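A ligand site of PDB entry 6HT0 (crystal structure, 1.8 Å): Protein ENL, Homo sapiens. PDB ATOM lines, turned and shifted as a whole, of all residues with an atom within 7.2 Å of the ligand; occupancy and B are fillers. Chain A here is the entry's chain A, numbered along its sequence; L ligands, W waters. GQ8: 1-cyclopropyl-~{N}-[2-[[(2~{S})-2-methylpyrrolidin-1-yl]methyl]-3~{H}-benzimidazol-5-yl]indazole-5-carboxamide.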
ATOM      1  N   GLU A  27     -20.156 -11.806  14.509  1.00  0.00           N
ATOM      2  CA  GLU A  27     -20.578 -11.295  15.843  1.00  0.00           C
ATOM      3  C   GLU A  27     -19.684 -11.841  16.968  1.00  0.00           C
ATOM      4  O   GLU A  27     -19.858 -11.375  18.137  1.00  0.00           O
ATOM      5  CB  GLU A  27     -22.039 -11.653  16.113  1.00  0.00           C
ATOM      6  CG  GLU A  27     -22.995 -11.150  15.044  1.00  0.00           C
ATOM      7  CD  GLU A  27     -23.445 -12.180  14.020  1.00  0.00           C
ATOM      8  OE1 GLU A  27     -22.820 -13.265  13.942  1.00  0.00           O
ATOM      9  OE2 GLU A  27     -24.417 -11.896  13.318  1.00  0.00           O
ATOM     10  N   PHE A  29     -19.710 -15.107  17.839  1.00  0.00           N
ATOM     11  CA  PHE A  29     -20.302 -16.367  18.346  1.00  0.00           C
ATOM     12  C   PHE A  29     -19.294 -17.483  18.042  1.00  0.00           C
ATOM     13  O   PHE A  29     -18.868 -17.615  16.900  1.00  0.00           O
ATOM     14  CB  PHE A  29     -21.661 -16.639  17.711  1.00  0.00           C
ATOM     15  CG  PHE A  29     -22.675 -15.546  17.896  1.00  0.00           C
ATOM     16  CD1 PHE A  29     -22.887 -14.949  19.119  1.00  0.00           C
ATOM     17  CD2 PHE A  29     -23.494 -15.167  16.834  1.00  0.00           C
ATOM     18  CE1 PHE A  29     -23.846 -13.972  19.278  1.00  0.00           C
ATOM     19  CE2 PHE A  29     -24.440 -14.174  17.001  1.00  0.00           C
ATOM     20  CZ  PHE A  29     -24.617 -13.582  18.230  1.00  0.00           C
ATOM     21  N   HIS A  31     -19.719 -20.800  19.044  1.00  0.00           N
ATOM     22  CA  HIS A  31     -20.313 -22.149  19.095  1.00  0.00           C
ATOM     23  C   HIS A  31     -21.644 -22.169  18.419  1.00  0.00           C
ATOM     24  O   HIS A  31     -22.349 -21.179  18.470  1.00  0.00           O
ATOM     25  CB  HIS A  31     -20.505 -22.624  20.549  1.00  0.00           C
ATOM     26  CG  HIS A  31     -19.265 -23.039  21.234  1.00  0.00           C
ATOM     27  ND1 HIS A  31     -18.341 -22.139  21.684  1.00  0.00           N
ATOM     28  CD2 HIS A  31     -18.831 -24.253  21.604  1.00  0.00           C
ATOM     29  CE1 HIS A  31     -17.387 -22.786  22.312  1.00  0.00           C
ATOM     30  NE2 HIS A  31     -17.671 -24.092  22.254  1.00  0.00           N
ATOM     31  N   TRP A  33     -25.088 -24.486  18.856  1.00  0.00           N
ATOM     32  CA  TRP A  33     -25.702 -25.484  19.750  1.00  0.00           C
ATOM     33  C   TRP A  33     -27.161 -25.720  19.364  1.00  0.00           C
ATOM     34  O   TRP A  33     -27.759 -24.925  18.584  1.00  0.00           O
ATOM     35  CB  TRP A  33     -25.530 -25.098  21.210  1.00  0.00           C
ATOM     36  CG  TRP A  33     -26.080 -23.769  21.639  1.00  0.00           C
ATOM     37  CD1 TRP A  33     -25.341 -22.661  21.928  1.00  0.00           C
ATOM     38  CD2 TRP A  33     -27.445 -23.436  21.927  1.00  0.00           C
ATOM     39  NE1 TRP A  33     -26.154 -21.652  22.357  1.00  0.00           N
ATOM     40  CE2 TRP A  33     -27.448 -22.100  22.369  1.00  0.00           C
ATOM     41  CE3 TRP A  33     -28.668 -24.136  21.868  1.00  0.00           C
ATOM     42  CZ2 TRP A  33     -28.618 -21.451  22.755  1.00  0.00           C
ATOM     43  CZ3 TRP A  33     -29.823 -23.476  22.243  1.00  0.00           C
ATOM     44  CH2 TRP A  33     -29.788 -22.154  22.661  1.00  0.00           C
ATOM     45  N   LEU A  56     -34.168 -19.037  26.935  1.00  0.00           N
ATOM     46  CA  LEU A  56     -32.761 -18.735  26.590  1.00  0.00           C
ATOM     47  C   LEU A  56     -32.244 -17.616  27.505  1.00  0.00           C
ATOM     48  O   LEU A  56     -33.056 -16.899  28.104  1.00  0.00           O
ATOM     49  CB  LEU A  56     -32.680 -18.320  25.128  1.00  0.00           C
ATOM     50  CG  LEU A  56     -32.565 -19.449  24.105  1.00  0.00           C
ATOM     51  CD1 LEU A  56     -33.654 -20.492  24.308  1.00  0.00           C
ATOM     52  CD2 LEU A  56     -32.603 -18.904  22.720  1.00  0.00           C
ATOM     53  N   HIS A  57     -30.946 -17.446  27.577  1.00  0.00           N
ATOM     54  CA  HIS A  57     -30.302 -16.339  28.313  1.00  0.00           C
ATOM     55  C   HIS A  57     -30.937 -15.023  27.819  1.00  0.00           C
ATOM     56  O   HIS A  57     -31.219 -14.951  26.601  1.00  0.00           O
ATOM     57  CB  HIS A  57     -28.802 -16.426  28.101  1.00  0.00           C
ATOM     58  CG  HIS A  57     -28.058 -15.450  28.925  1.00  0.00           C
ATOM     59  ND1 HIS A  57     -27.809 -14.191  28.491  1.00  0.00           N
ATOM     60  CD2 HIS A  57     -27.543 -15.542  30.156  1.00  0.00           C
ATOM     61  CE1 HIS A  57     -27.162 -13.531  29.417  1.00  0.00           C
ATOM     62  NE2 HIS A  57     -26.984 -14.340  30.441  1.00  0.00           N
ATOM     63  N   ASP A  58     -31.185 -14.049  28.721  1.00  0.00           N
ATOM     64  CA  ASP A  58     -31.915 -12.764  28.442  1.00  0.00           C
ATOM     65  C   ASP A  58     -31.238 -11.994  27.293  1.00  0.00           C
ATOM     66  O   ASP A  58     -31.924 -11.160  26.659  1.00  0.00           O
ATOM     67  CB  ASP A  58     -32.008 -11.856  29.682  1.00  0.00           C
ATOM     68  CG  ASP A  58     -32.837 -12.383  30.864  1.00  0.00           C
ATOM     69  OD1 ASP A  58     -33.697 -13.243  30.651  1.00  0.00           O
ATOM     70  OD2 ASP A  58     -32.618 -11.903  32.014  1.00  0.00           O
ATOM     71  N   SER A  59     -29.959 -12.256  26.996  1.00  0.00           N
ATOM     72  CA  SER A  59     -29.198 -11.621  25.892  1.00  0.00           C
ATOM     73  C   SER A  59     -29.728 -12.005  24.513  1.00  0.00           C
ATOM     74  O   SER A  59     -29.475 -11.261  23.590  1.00  0.00           O
ATOM     75  CB  SER A  59     -27.727 -11.952  25.981  1.00  0.00           C
ATOM     76  OG  SER A  59     -27.536 -13.346  25.962  1.00  0.00           O
ATOM     77  N   PHE A  60     -30.383 -13.149  24.368  1.00  0.00           N
ATOM     78  CA  PHE A  60     -30.856 -13.663  23.082  1.00  0.00           C
ATOM     79  C   PHE A  60     -32.055 -12.872  22.636  1.00  0.00           C
ATOM     80  O   PHE A  60     -32.851 -12.465  23.474  1.00  0.00           O
ATOM     81  CB  PHE A  60     -31.253 -15.149  23.172  1.00  0.00           C
ATOM     82  CG  PHE A  60     -30.095 -16.090  23.070  1.00  0.00           C
ATOM     83  CD1 PHE A  60     -29.355 -16.424  24.193  1.00  0.00           C
ATOM     84  CD2 PHE A  60     -29.742 -16.630  21.848  1.00  0.00           C
ATOM     85  CE1 PHE A  60     -28.284 -17.305  24.096  1.00  0.00           C
ATOM     86  CE2 PHE A  60     -28.670 -17.499  21.737  1.00  0.00           C
ATOM     87  CZ  PHE A  60     -27.944 -17.833  22.860  1.00  0.00           C
ATOM     88  N   PRO A  61     -32.215 -12.634  21.327  1.00  0.00           N
ATOM     89  CA  PRO A  61     -33.459 -12.063  20.819  1.00  0.00           C
ATOM     90  C   PRO A  61     -34.572 -13.084  21.106  1.00  0.00           C
ATOM     91  O   PRO A  61     -34.316 -14.260  20.976  1.00  0.00           O
ATOM     92  CB  PRO A  61     -33.184 -11.849  19.319  1.00  0.00           C
ATOM     93  CG  PRO A  61     -32.084 -12.848  18.995  1.00  0.00           C
ATOM     94  CD  PRO A  61     -31.252 -12.942  20.255  1.00  0.00           C
ATOM     95  N   ARG A  65     -38.617 -19.111  23.668  1.00  0.00           N
ATOM     96  CA  ARG A  65     -38.731 -19.842  22.398  1.00  0.00           C
ATOM     97  C   ARG A  65     -39.759 -20.921  22.576  1.00  0.00           C
ATOM     98  O   ARG A  65     -39.566 -21.798  23.422  1.00  0.00           O
ATOM     99  CB  ARG A  65     -37.366 -20.395  21.969  1.00  0.00           C
ATOM    100  CG  ARG A  65     -36.314 -19.338  21.707  1.00  0.00           C
ATOM    101  CD  ARG A  65     -36.638 -18.370  20.561  1.00  0.00           C
ATOM    102  NE  ARG A  65     -35.552 -17.415  20.526  1.00  0.00           N
ATOM    103  CZ  ARG A  65     -34.384 -17.606  19.938  1.00  0.00           C
ATOM    104  NH1 ARG A  65     -34.137 -18.719  19.259  1.00  0.00           N
ATOM    105  NH2 ARG A  65     -33.439 -16.678  20.018  1.00  0.00           N
ATOM    106  N   GLU A  75     -32.192 -24.192  17.740  1.00  0.00           N
ATOM    107  CA  GLU A  75     -30.849 -24.176  17.139  1.00  0.00           C
ATOM    108  C   GLU A  75     -30.332 -22.739  17.254  1.00  0.00           C
ATOM    109  O   GLU A  75     -31.047 -21.804  16.839  1.00  0.00           O
ATOM    110  CB  GLU A  75     -30.899 -24.653  15.697  1.00  0.00           C
ATOM    111  CG  GLU A  75     -31.330 -26.076  15.579  1.00  0.00           C
ATOM    112  CD  GLU A  75     -31.540 -26.561  14.161  1.00  0.00           C
ATOM    113  OE1 GLU A  75     -32.550 -26.172  13.521  1.00  0.00           O
ATOM    114  OE2 GLU A  75     -30.695 -27.306  13.709  1.00  0.00           O
ATOM    115  N   GLU A  76     -29.154 -22.567  17.809  1.00  0.00           N
ATOM    116  CA  GLU A  76     -28.601 -21.229  17.995  1.00  0.00           C
ATOM    117  C   GLU A  76     -27.101 -21.253  17.830  1.00  0.00           C
ATOM    118  O   GLU A  76     -26.511 -22.299  17.675  1.00  0.00           O
ATOM    119  CB  GLU A  76     -28.986 -20.707  19.373  1.00  0.00           C
ATOM    120  CG  GLU A  76     -30.224 -19.868  19.389  1.00  0.00           C
ATOM    121  CD  GLU A  76     -30.138 -18.552  18.691  1.00  0.00           C
ATOM    122  OE1 GLU A  76     -29.001 -18.219  18.149  1.00  0.00           O
ATOM    123  OE2 GLU A  76     -31.156 -17.819  18.730  1.00  0.00           O
ATOM    124  N   SER A  77     -26.547 -20.075  17.797  1.00  0.00           N
ATOM    125  CA  SER A  77     -25.083 -19.874  17.964  1.00  0.00           C
ATOM    126  C   SER A  77     -24.896 -18.979  19.189  1.00  0.00           C
ATOM    127  O   SER A  77     -25.855 -18.283  19.588  1.00  0.00           O
ATOM    128  CB  SER A  77     -24.423 -19.345  16.699  1.00  0.00           C
ATOM    129  OG  SER A  77     -24.307 -20.384  15.715  1.00  0.00           O
ATOM    130  N   GLY A  78     -23.762 -19.067  19.808  1.00  0.00           N
ATOM    131  CA  GLY A  78     -23.609 -18.322  21.047  1.00  0.00           C
ATOM    132  C   GLY A  78     -22.183 -18.298  21.515  1.00  0.00           C
ATOM    133  O   GLY A  78     -21.286 -18.884  20.830  1.00  0.00           O
ATOM    134  N   TYR A  79     -21.986 -17.639  22.647  1.00  0.00           N
ATOM    135  CA  TYR A  79     -20.639 -17.380  23.201  1.00  0.00           C
ATOM    136  C   TYR A  79     -20.377 -18.282  24.374  1.00  0.00           C
ATOM    137  O   TYR A  79     -19.214 -18.447  24.755  1.00  0.00           O
ATOM    138  CB  TYR A  79     -20.515 -15.959  23.750  1.00  0.00           C
ATOM    139  CG  TYR A  79     -20.947 -14.828  22.892  1.00  0.00           C
ATOM    140  CD1 TYR A  79     -20.128 -14.368  21.873  1.00  0.00           C
ATOM    141  CD2 TYR A  79     -22.100 -14.109  23.179  1.00  0.00           C
ATOM    142  CE1 TYR A  79     -20.476 -13.268  21.095  1.00  0.00           C
ATOM    143  CE2 TYR A  79     -22.472 -13.011  22.420  1.00  0.00           C
ATOM    144  CZ  TYR A  79     -21.641 -12.582  21.368  1.00  0.00           C
ATOM    145  OH  TYR A  79     -21.981 -11.520  20.581  1.00  0.00           O
ATOM    146  N   ALA A  80     -21.424 -18.790  25.035  1.00  0.00           N
ATOM    147  CA  ALA A  80     -21.280 -19.378  26.371  1.00  0.00           C
ATOM    148  C   ALA A  80     -22.494 -20.234  26.697  1.00  0.00           C
ATOM    149  O   ALA A  80     -23.574 -19.921  26.245  1.00  0.00           O
ATOM    150  CB  ALA A  80     -21.100 -18.305  27.382  1.00  0.00           C
ATOM    151  N   GLY A  81     -22.263 -21.257  27.492  1.00  0.00           N
ATOM    152  CA  GLY A  81     -23.276 -22.113  28.051  1.00  0.00           C
ATOM    153  C   GLY A  81     -24.050 -21.397  29.123  1.00  0.00           C
ATOM    154  O   GLY A  81     -23.594 -20.350  29.591  1.00  0.00           O
ATOM    155  N   PHE A  82     -25.180 -21.928  29.520  1.00  0.00           N
ATOM    156  CA  PHE A  82     -26.019 -21.323  30.561  1.00  0.00           C
ATOM    157  C   PHE A  82     -27.016 -22.350  31.020  1.00  0.00           C
ATOM    158  O   PHE A  82     -27.130 -23.397  30.364  1.00  0.00           O
ATOM    159  CB  PHE A  82     -26.708 -20.041  30.048  1.00  0.00           C
ATOM    160  CG  PHE A  82     -27.536 -20.205  28.805  1.00  0.00           C
ATOM    161  CD1 PHE A  82     -26.968 -20.039  27.550  1.00  0.00           C
ATOM    162  CD2 PHE A  82     -28.897 -20.534  28.881  1.00  0.00           C
ATOM    163  CE1 PHE A  82     -27.737 -20.193  26.404  1.00  0.00           C
ATOM    164  CE2 PHE A  82     -29.652 -20.674  27.734  1.00  0.00           C
ATOM    165  CZ  PHE A  82     -29.071 -20.518  26.494  1.00  0.00           C
ATOM    166  N   ILE A  83     -27.697 -22.041  32.106  1.00  0.00           N
ATOM    167  CA  ILE A  83     -28.780 -22.871  32.649  1.00  0.00           C
ATOM    168  C   ILE A  83     -30.067 -22.420  31.990  1.00  0.00           C
ATOM    169  O   ILE A  83     -30.416 -21.229  32.063  1.00  0.00           O
ATOM    170  CB  ILE A  83     -28.857 -22.782  34.167  1.00  0.00           C
ATOM    171  CG1 ILE A  83     -27.534 -23.187  34.808  1.00  0.00           C
ATOM    172  CG2 ILE A  83     -30.005 -23.613  34.650  1.00  0.00           C
ATOM    173  CD1 ILE A  83     -27.034 -24.535  34.388  1.00  0.00           C
ATOM    174  N   LEU A 107     -21.156 -25.873  26.772  1.00  0.00           N
ATOM    175  CA  LEU A 107     -20.457 -25.916  25.473  1.00  0.00           C
ATOM    176  C   LEU A 107     -19.124 -26.608  25.659  1.00  0.00           C
ATOM    177  O   LEU A 107     -18.692 -26.713  26.811  1.00  0.00           O
ATOM    178  CB  LEU A 107     -20.270 -24.474  24.984  1.00  0.00           C
ATOM    179  CG  LEU A 107     -21.519 -23.638  24.905  1.00  0.00           C
ATOM    180  CD1 LEU A 107     -21.187 -22.288  24.291  1.00  0.00           C
ATOM    181  CD2 LEU A 107     -22.625 -24.326  24.139  1.00  0.00           C
HETATM  182  C1  GQ8 L   1     -29.487 -16.467  15.406  1.00  0.00           C
HETATM  183  C2  GQ8 L   1     -30.998 -16.703  15.471  1.00  0.00           C
HETATM  184  C3  GQ8 L   1     -31.510 -15.621  16.355  1.00  0.00           C
HETATM  185  N4  GQ8 L   1     -23.751 -15.075  29.724  1.00  0.00           N
HETATM  186  C5  GQ8 L   1     -27.867 -15.370  16.887  1.00  0.00           C
HETATM  187  C6  GQ8 L   1     -27.540 -15.005  18.299  1.00  0.00           C
HETATM  188  C8  GQ8 L   1     -26.270 -15.337  21.547  1.00  0.00           C
HETATM  189  C9  GQ8 L   1     -26.404 -14.428  22.594  1.00  0.00           C
HETATM  190  C10 GQ8 L   1     -25.087 -15.647  24.321  1.00  0.00           C
HETATM  191  C11 GQ8 L   1     -24.693 -15.532  25.754  1.00  0.00           C
HETATM  192  C13 GQ8 L   1     -24.253 -16.341  27.965  1.00  0.00           C
HETATM  193  C15 GQ8 L   1     -23.597 -13.948  30.635  1.00  0.00           C
HETATM  194  C16 GQ8 L   1     -22.377 -13.100  30.499  1.00  0.00           C
HETATM  195  C18 GQ8 L   1     -24.062 -15.018  28.392  1.00  0.00           C
HETATM  196  C19 GQ8 L   1     -24.162 -13.968  27.512  1.00  0.00           C
HETATM  197  C21 GQ8 L   1     -27.064 -13.205  22.392  1.00  0.00           C
HETATM  198  C22 GQ8 L   1     -27.605 -12.886  21.161  1.00  0.00           C
HETATM  199  C23 GQ8 L   1     -27.488 -13.817  20.139  1.00  0.00           C
HETATM  200  O   GQ8 L   1     -24.643 -16.551  23.612  1.00  0.00           O
HETATM  201  C20 GQ8 L   1     -24.468 -14.227  26.200  1.00  0.00           C
HETATM  202  C17 GQ8 L   1     -22.527 -14.013  31.677  1.00  0.00           C
HETATM  203  N3  GQ8 L   1     -23.709 -16.369  30.171  1.00  0.00           N
HETATM  204  C14 GQ8 L   1     -24.014 -17.120  29.134  1.00  0.00           C
HETATM  205  C12 GQ8 L   1     -24.585 -16.603  26.640  1.00  0.00           C
HETATM  206  N2  GQ8 L   1     -25.885 -14.645  23.879  1.00  0.00           N
HETATM  207  C7  GQ8 L   1     -26.825 -15.032  20.318  1.00  0.00           C
HETATM  208  N1  GQ8 L   1     -26.872 -15.763  19.140  1.00  0.00           N
HETATM  209  N5  GQ8 L   1     -27.935 -13.831  18.839  1.00  0.00           N
HETATM  210  N   GQ8 L   1     -29.179 -16.016  16.782  1.00  0.00           N
HETATM  211  C   GQ8 L   1     -28.705 -17.688  14.977  1.00  0.00           C
HETATM  212  C4  GQ8 L   1     -30.287 -15.105  17.138  1.00  0.00           C
HETATM  213  O   HOH W   1     -25.008 -19.378  23.942  1.00  0.00           O
HETATM  214  O   HOH W   2     -23.660 -16.978  32.522  1.00  0.00           O
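NE2 of His 57 sits close to N4 of the ligand, 3.4 Å away. Merely in contact with the ligand: Phe 60 (3.2 Å), Phe 29 (3.3 Å), Gly 78 (3.3 Å), Gly 81 (3.3 Å), Pro 61 (3.4 Å) and Ala 80 (3.5 Å). 11 residues have an atom within 4 Å of the ligand: Phe 29, His 57, Ser 59, Phe 60, Pro 61, Glu 76, Ser 77, Gly 78, Tyr 79, Ala 80 and Gly 81. The nearest printed residue that does not touch the ligand is Phe 82 (4.1 Å).
Water W1 lies within hydrogen-bond range of the backbone carbonyl oxygen of Ala 80 (2.8 Å), an oxygen (O) of the ligand (2.9 Å) and the indole nitrogen of Trp 33 (3.0 Å).
OE2 of Glu 76 is in salt-bridge range of NH2 of Arg 65. The backbone NH (N) of Glu 76 is in hydrogen-bond range of the backbone carbonyl oxygen (O) of Trp 33 (2.8 Å). OG of Ser 77 lies close to O of His 31 (3.5 Å). OG of Ser 59 lies within hydrogen-bond range of ND1 of His 57, at 2.7 Å. The side-chain hydroxyl (OH) of Tyr 79 sits at hydrogen-bond distance from the backbone carbonyl oxygen (O) of Glu 27 (3.2 Å). The backbone NH (N) of Gly 78 is in hydrogen-bond range of the backbone carbonyl oxygen (O) of His 31 (2.9 Å). NH2 of Arg 65 lies within hydrogen-bond range of O of Pro 61.
OE1 of Glu 76 is in salt-bridge range of N of the ligand. O of Ser 77 is in hydrogen-bond range of N1 of the ligand, 2.8 Å away. OG of Ser 59 is in hydrogen-bond range of N2 of the ligand, 3.0 Å away. The backbone NH (N) of Tyr 79 lies within hydrogen-bond range of an oxygen (O) of the ligand, 3.0 Å away.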
